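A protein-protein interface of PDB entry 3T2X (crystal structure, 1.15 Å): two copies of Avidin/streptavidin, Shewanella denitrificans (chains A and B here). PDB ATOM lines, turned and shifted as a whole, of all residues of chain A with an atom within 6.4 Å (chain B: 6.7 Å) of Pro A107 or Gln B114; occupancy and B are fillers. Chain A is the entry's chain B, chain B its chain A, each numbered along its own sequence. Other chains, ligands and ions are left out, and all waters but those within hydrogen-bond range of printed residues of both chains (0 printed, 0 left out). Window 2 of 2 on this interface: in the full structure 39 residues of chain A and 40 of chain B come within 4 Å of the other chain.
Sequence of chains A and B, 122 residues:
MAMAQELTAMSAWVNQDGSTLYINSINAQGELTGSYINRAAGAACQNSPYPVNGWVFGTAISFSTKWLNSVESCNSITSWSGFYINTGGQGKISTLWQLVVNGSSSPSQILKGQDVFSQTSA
The backbone carbonyl oxygen of Gln B114 sits at hydrogen-bond distance from the side-chain amide nitrogen of Gln B16, 3.2 Å away.
N of Ser B94 is in hydrogen-bond range of O of Phe B83, 2.9 Å away.
The backbone NH (N) of Ser A105 is in hydrogen-bond range of the side-chain amide oxygen (OE1) of Gln A109.
The side-chain hydroxyl (OG) of Ser A108 sits at hydrogen-bond distance from the side-chain hydroxyl (OG) of Ser A106.
The backbone NH (N) of Ser A106 is in hydrogen-bond range of the side-chain amide oxygen (OE1) of Gln A109, at 3.1 Å.
Of the 8 printed residues of chain A, 5 touch a printed residue of chain B.
Of the 12 printed residues of chain B, 4 touch a printed residue of chain A.
Printed residues of chain B that touch a printed residue of chain A: Phe B83, Ser B94, Leu B96 and Gln B114.
Among the printed residues, 7 pairs touch across the chains.
Among the printed residues, no Asp or Glu carboxylate lies within 4 Å of a Lys or Arg side-chain nitrogen of the other chain.
CE2 of Phe B83 touches C of Ser A105, at 3.4 Å.
N of Ser A106 touches CZ of Phe B83, at 3.4 Å.
Pro A107 touches Phe B83.
Ser B94 touches Pro A107.
Gln B114 touches Pro A107 (NE2 to CG, 3.9 Å).
CG of Leu B96 touches CD1 of Ile A110 (3.998 Å).
Lys A112 touches Leu B96 (CE to CD1, 3.7 Å).
Of chain B, only Phe B83 (3.5 Å), Ser B94 (3.8 Å) and Gln B114 (3.9 Å) come within 4 Å of Pro A107.
Of the printed residues of chain B, Ile A110 touches Leu B96.
Of the printed residues of chain A, Leu B96 touches Ile A110 and Lys A112.
Gln A109 touches none of the printed residues of chain B.
Lys B112 touches none of the printed residues of chain A.
Position printed for both chains: 112.
Of the 7 pairs that touch across the chains among the printed residues, none has its exchanged pair printed and touching as well.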
ATOM      1  N   SER A 105      23.737   1.487   5.486  1.00  0.00           N
ATOM      2  CA  SER A 105      23.865   0.130   4.929  1.00  0.00           C
ATOM      3  C   SER A 105      22.774  -0.195   3.915  1.00  0.00           C
ATOM      4  O   SER A 105      22.858  -1.222   3.253  1.00  0.00           O
ATOM      5  CB  SER A 105      23.823  -0.916   6.045  1.00  0.00           C
ATOM      6  OG  SER A 105      22.632  -0.755   6.763  1.00  0.00           O
ATOM      7  N   SER A 106      21.753   0.649   3.803  1.00  0.00           N
ATOM      8  CA  SER A 106      20.632   0.360   2.902  1.00  0.00           C
ATOM      9  C   SER A 106      20.115   1.637   2.246  1.00  0.00           C
ATOM     10  O   SER A 106      20.063   2.664   2.911  1.00  0.00           O
ATOM     11  CB  SER A 106      19.489  -0.275   3.702  1.00  0.00           C
ATOM     12  OG  SER A 106      18.340  -0.349   2.884  1.00  0.00           O
ATOM     13  N   PRO A 107      19.684   1.583   0.964  1.00  0.00           N
ATOM     14  CA  PRO A 107      19.102   2.769   0.350  1.00  0.00           C
ATOM     15  C   PRO A 107      17.839   3.241   1.053  1.00  0.00           C
ATOM     16  O   PRO A 107      17.497   4.415   0.927  1.00  0.00           O
ATOM     17  CB  PRO A 107      18.774   2.316  -1.085  1.00  0.00           C
ATOM     18  CG  PRO A 107      19.572   1.129  -1.310  1.00  0.00           C
ATOM     19  CD  PRO A 107      19.717   0.455   0.012  1.00  0.00           C
ATOM     20  N   SER A 108      17.160   2.362   1.801  1.00  0.00           N
ATOM     21  CA  SER A 108      15.985   2.812   2.556  1.00  0.00           C
ATOM     22  C   SER A 108      16.323   3.842   3.630  1.00  0.00           C
ATOM     23  O   SER A 108      15.420   4.492   4.156  1.00  0.00           O
ATOM     24  CB  SER A 108      15.278   1.632   3.224  1.00  0.00           C
ATOM     25  OG  SER A 108      16.142   1.059   4.191  1.00  0.00           O
ATOM     26  N   GLN A 109      17.610   3.972   3.962  1.00  0.00           N
ATOM     27  CA  GLN A 109      18.063   4.939   4.961  1.00  0.00           C
ATOM     28  C   GLN A 109      18.338   6.311   4.372  1.00  0.00           C
ATOM     29  O   GLN A 109      18.609   7.265   5.123  1.00  0.00           O
ATOM     30  CB  GLN A 109      19.325   4.424   5.636  1.00  0.00           C
ATOM     31  CG  GLN A 109      19.045   3.183   6.475  1.00  0.00           C
ATOM     32  CD  GLN A 109      20.283   2.546   6.968  1.00  0.00           C
ATOM     33  OE1 GLN A 109      21.274   2.479   6.265  1.00  0.00           O
ATOM     34  NE2 GLN A 109      20.241   2.068   8.213  1.00  0.00           N
ATOM     35  N   ILE A 110      18.286   6.421   3.048  1.00  0.00           N
ATOM     36  CA  ILE A 110      18.450   7.731   2.395  1.00  0.00           C
ATOM     37  C   ILE A 110      17.112   8.482   2.542  1.00  0.00           C
ATOM     38  O   ILE A 110      16.063   7.962   2.166  1.00  0.00           O
ATOM     39  CB  ILE A 110      18.861   7.544   0.939  1.00  0.00           C
ATOM     40  CG1 ILE A 110      20.252   6.908   0.881  1.00  0.00           C
ATOM     41  CG2 ILE A 110      18.871   8.913   0.167  1.00  0.00           C
ATOM     42  CD1 ILE A 110      20.689   6.486  -0.515  1.00  0.00           C
ATOM     43  N   LEU A 111      17.132   9.643   3.182  1.00  0.00           N
ATOM     44  CA  LEU A 111      15.922  10.414   3.447  1.00  0.00           C
ATOM     45  C   LEU A 111      15.629  11.271   2.210  1.00  0.00           C
ATOM     46  O   LEU A 111      16.533  11.742   1.532  1.00  0.00           O
ATOM     47  CB  LEU A 111      16.135  11.307   4.684  1.00  0.00           C
ATOM     48  CG  LEU A 111      16.485  10.624   6.015  1.00  0.00           C
ATOM     49  CD1 LEU A 111      16.569  11.639   7.174  1.00  0.00           C
ATOM     50  CD2 LEU A 111      15.511   9.503   6.338  1.00  0.00           C
ATOM     51  N   LYS A 112      14.349  11.467   1.938  1.00  0.00           N
ATOM     52  CA  LYS A 112      13.907  12.218   0.757  1.00  0.00           C
ATOM     53  C   LYS A 112      12.901  13.248   1.173  1.00  0.00           C
ATOM     54  O   LYS A 112      12.062  12.990   2.045  1.00  0.00           O
ATOM     55  CB  LYS A 112      13.248  11.281  -0.259  1.00  0.00           C
ATOM     56  CG  LYS A 112      14.167  10.263  -0.950  1.00  0.00           C
ATOM     57  CD  LYS A 112      13.358   9.432  -1.955  1.00  0.00           C
ATOM     58  CE  LYS A 112      14.104   8.214  -2.416  1.00  0.00           C
ATOM     59  NZ  LYS A 112      13.199   7.395  -3.274  1.00  0.00           N
ATOM     60  N   GLN B  16      25.680  -0.555 -13.315  1.00  0.00           N
ATOM     61  CA  GLN B  16      25.038  -1.711 -13.940  1.00  0.00           C
ATOM     62  C   GLN B  16      24.834  -1.518 -15.437  1.00  0.00           C
ATOM     63  O   GLN B  16      24.640  -2.482 -16.147  1.00  0.00           O
ATOM     64  CB  GLN B  16      23.693  -2.008 -13.251  1.00  0.00           C
ATOM     65  CG  GLN B  16      22.543  -1.043 -13.541  1.00  0.00           C
ATOM     66  CD  GLN B  16      22.577   0.251 -12.733  1.00  0.00           C
ATOM     67  OE1 GLN B  16      23.535   0.580 -12.015  1.00  0.00           O
ATOM     68  NE2 GLN B  16      21.510   1.002 -12.857  1.00  0.00           N
ATOM     69  N   TRP B  80      23.615  12.057  -7.824  1.00  0.00           N
ATOM     70  CA  TRP B  80      23.579  10.796  -7.109  1.00  0.00           C
ATOM     71  C   TRP B  80      23.865  11.034  -5.635  1.00  0.00           C
ATOM     72  O   TRP B  80      24.757  11.819  -5.265  1.00  0.00           O
ATOM     73  CB  TRP B  80      24.675   9.861  -7.646  1.00  0.00           C
ATOM     74  CG  TRP B  80      24.498   9.298  -9.039  1.00  0.00           C
ATOM     75  CD1 TRP B  80      24.030   8.069  -9.352  1.00  0.00           C
ATOM     76  CD2 TRP B  80      24.860   9.928 -10.274  1.00  0.00           C
ATOM     77  NE1 TRP B  80      24.088   7.863 -10.716  1.00  0.00           N
ATOM     78  CE2 TRP B  80      24.591   9.006 -11.305  1.00  0.00           C
ATOM     79  CE3 TRP B  80      25.435  11.167 -10.599  1.00  0.00           C
ATOM     80  CZ2 TRP B  80      24.888   9.282 -12.643  1.00  0.00           C
ATOM     81  CZ3 TRP B  80      25.725  11.441 -11.924  1.00  0.00           C
ATOM     82  CH2 TRP B  80      25.457  10.502 -12.932  1.00  0.00           C
ATOM     83  N   PHE B  83      26.104   5.546  -0.683  1.00  0.00           N
ATOM     84  CA  PHE B  83      26.971   5.117   0.425  1.00  0.00           C
ATOM     85  C   PHE B  83      27.835   3.964  -0.053  1.00  0.00           C
ATOM     86  O   PHE B  83      27.441   3.132  -0.872  1.00  0.00           O
ATOM     87  CB  PHE B  83      26.146   4.733   1.692  1.00  0.00           C
ATOM     88  CG  PHE B  83      25.119   3.679   1.438  1.00  0.00           C
ATOM     89  CD1 PHE B  83      23.849   3.994   0.979  1.00  0.00           C
ATOM     90  CD2 PHE B  83      25.446   2.343   1.654  1.00  0.00           C
ATOM     91  CE1 PHE B  83      22.924   2.983   0.694  1.00  0.00           C
ATOM     92  CE2 PHE B  83      24.534   1.330   1.404  1.00  0.00           C
ATOM     93  CZ  PHE B  83      23.287   1.645   0.904  1.00  0.00           C
ATOM     94  N   SER B  94      26.387   2.321  -3.460  1.00  0.00           N
ATOM     95  CA  SER B  94      24.971   2.128  -3.706  1.00  0.00           C
ATOM     96  C   SER B  94      24.285   3.489  -3.706  1.00  0.00           C
ATOM     97  O   SER B  94      24.430   4.217  -2.726  1.00  0.00           O
ATOM     98  CB  SER B  94      24.393   1.233  -2.621  1.00  0.00           C
ATOM     99  OG  SER B  94      23.008   1.061  -2.835  1.00  0.00           O
ATOM    100  N   THR B  95      23.593   3.822  -4.793  1.00  0.00           N
ATOM    101  CA  THR B  95      23.095   5.181  -4.975  1.00  0.00           C
ATOM    102  C   THR B  95      21.640   5.231  -5.388  1.00  0.00           C
ATOM    103  O   THR B  95      21.081   4.284  -5.963  1.00  0.00           O
ATOM    104  CB  THR B  95      23.864   5.981  -6.100  1.00  0.00           C
ATOM    105  OG1 THR B  95      23.491   5.485  -7.383  1.00  0.00           O
ATOM    106  CG2 THR B  95      25.387   5.920  -5.911  1.00  0.00           C
ATOM    107  N   LEU B  96      21.044   6.374  -5.081  1.00  0.00           N
ATOM    108  CA  LEU B  96      19.788   6.817  -5.698  1.00  0.00           C
ATOM    109  C   LEU B  96      20.105   8.094  -6.448  1.00  0.00           C
ATOM    110  O   LEU B  96      20.838   8.937  -5.918  1.00  0.00           O
ATOM    111  CB  LEU B  96      18.732   7.128  -4.615  1.00  0.00           C
ATOM    112  CG  LEU B  96      18.340   5.951  -3.705  1.00  0.00           C
ATOM    113  CD1 LEU B  96      17.287   6.364  -2.679  1.00  0.00           C
ATOM    114  CD2 LEU B  96      17.857   4.754  -4.507  1.00  0.00           C
ATOM    115  N   TRP B  97      19.544   8.264  -7.644  1.00  0.00           N
ATOM    116  CA  TRP B  97      19.825   9.443  -8.426  1.00  0.00           C
ATOM    117  C   TRP B  97      18.542  10.188  -8.787  1.00  0.00           C
ATOM    118  O   TRP B  97      17.439   9.613  -8.819  1.00  0.00           O
ATOM    119  CB  TRP B  97      20.674   9.103  -9.667  1.00  0.00           C
ATOM    120  CG  TRP B  97      20.093   8.085 -10.600  1.00  0.00           C
ATOM    121  CD1 TRP B  97      20.451   6.779 -10.655  1.00  0.00           C
ATOM    122  CD2 TRP B  97      19.084   8.264 -11.607  1.00  0.00           C
ATOM    123  NE1 TRP B  97      19.753   6.121 -11.628  1.00  0.00           N
ATOM    124  CE2 TRP B  97      18.925   7.021 -12.242  1.00  0.00           C
ATOM    125  CE3 TRP B  97      18.326   9.366 -12.061  1.00  0.00           C
ATOM    126  CZ2 TRP B  97      18.011   6.815 -13.274  1.00  0.00           C
ATOM    127  CZ3 TRP B  97      17.434   9.164 -13.108  1.00  0.00           C
ATOM    128  CH2 TRP B  97      17.293   7.898 -13.703  1.00  0.00           C
ATOM    129  N   LYS B 112      13.954   9.687 -11.531  1.00  0.00           N
ATOM    130  CA  LYS B 112      14.645   9.034 -10.421  1.00  0.00           C
ATOM    131  C   LYS B 112      15.028   7.611 -10.770  1.00  0.00           C
ATOM    132  O   LYS B 112      14.358   6.943 -11.552  1.00  0.00           O
ATOM    133  CB  LYS B 112      13.755   8.985  -9.175  1.00  0.00           C
ATOM    134  CG  LYS B 112      13.198  10.319  -8.708  1.00  0.00           C
ATOM    135  CD  LYS B 112      12.332  10.067  -7.473  1.00  0.00           C
ATOM    136  CE  LYS B 112      11.937  11.348  -6.774  1.00  0.00           C
ATOM    137  NZ  LYS B 112      10.597  11.741  -7.259  1.00  0.00           N
ATOM    138  N   GLY B 113      16.102   7.120 -10.162  1.00  0.00           N
ATOM    139  CA  GLY B 113      16.464   5.711 -10.302  1.00  0.00           C
ATOM    140  C   GLY B 113      17.494   5.314  -9.279  1.00  0.00           C
ATOM    141  O   GLY B 113      17.835   6.073  -8.354  1.00  0.00           O
ATOM    142  N   GLN B 114      18.033   4.121  -9.494  1.00  0.00           N
ATOM    143  CA  GLN B 114      18.932   3.472  -8.555  1.00  0.00           C
ATOM    144  C   GLN B 114      20.096   2.874  -9.342  1.00  0.00           C
ATOM    145  O   GLN B 114      19.881   2.155 -10.306  1.00  0.00           O
ATOM    146  CB  GLN B 114      18.133   2.373  -7.835  1.00  0.00           C
ATOM    147  CG  GLN B 114      18.833   1.645  -6.750  1.00  0.00           C
ATOM    148  CD  GLN B 114      17.957   0.623  -5.977  1.00  0.00           C
ATOM    149  OE1 GLN B 114      16.829   0.280  -6.368  1.00  0.00           O
ATOM    150  NE2 GLN B 114      18.500   0.135  -4.874  1.00  0.00           N
ATOM    151  N   ASP B 115      21.329   3.173  -8.934  1.00  0.00           N
ATOM    152  CA  ASP B 115      22.520   2.620  -9.590  1.00  0.00           C
ATOM    153  C   ASP B 115      23.461   2.099  -8.490  1.00  0.00           C
ATOM    154  O   ASP B 115      23.626   2.745  -7.457  1.00  0.00           O
ATOM    155  CB  ASP B 115      23.335   3.732 -10.290  1.00  0.00           C
ATOM    156  CG  ASP B 115      22.709   4.322 -11.548  1.00  0.00           C
ATOM    157  OD1 ASP B 115      21.691   3.832 -12.058  1.00  0.00           O
ATOM    158  OD2 ASP B 115      23.345   5.289 -12.041  1.00  0.00           O
ATOM    159  N   VAL B 116      24.159   0.989  -8.751  1.00  0.00           N
ATOM    160  CA  VAL B 116      25.267   0.595  -7.911  1.00  0.00           C
ATOM    161  C   VAL B 116      26.527   0.628  -8.751  1.00  0.00           C
ATOM    162  O   VAL B 116      26.586   0.027  -9.827  1.00  0.00           O
ATOM    163  CB  VAL B 116      25.066  -0.814  -7.300  1.00  0.00           C
ATOM    164  CG1 VAL B 116      26.302  -1.217  -6.488  1.00  0.00           C
ATOM    165  CG2 VAL B 116      23.787  -0.836  -6.467  1.00  0.00           C
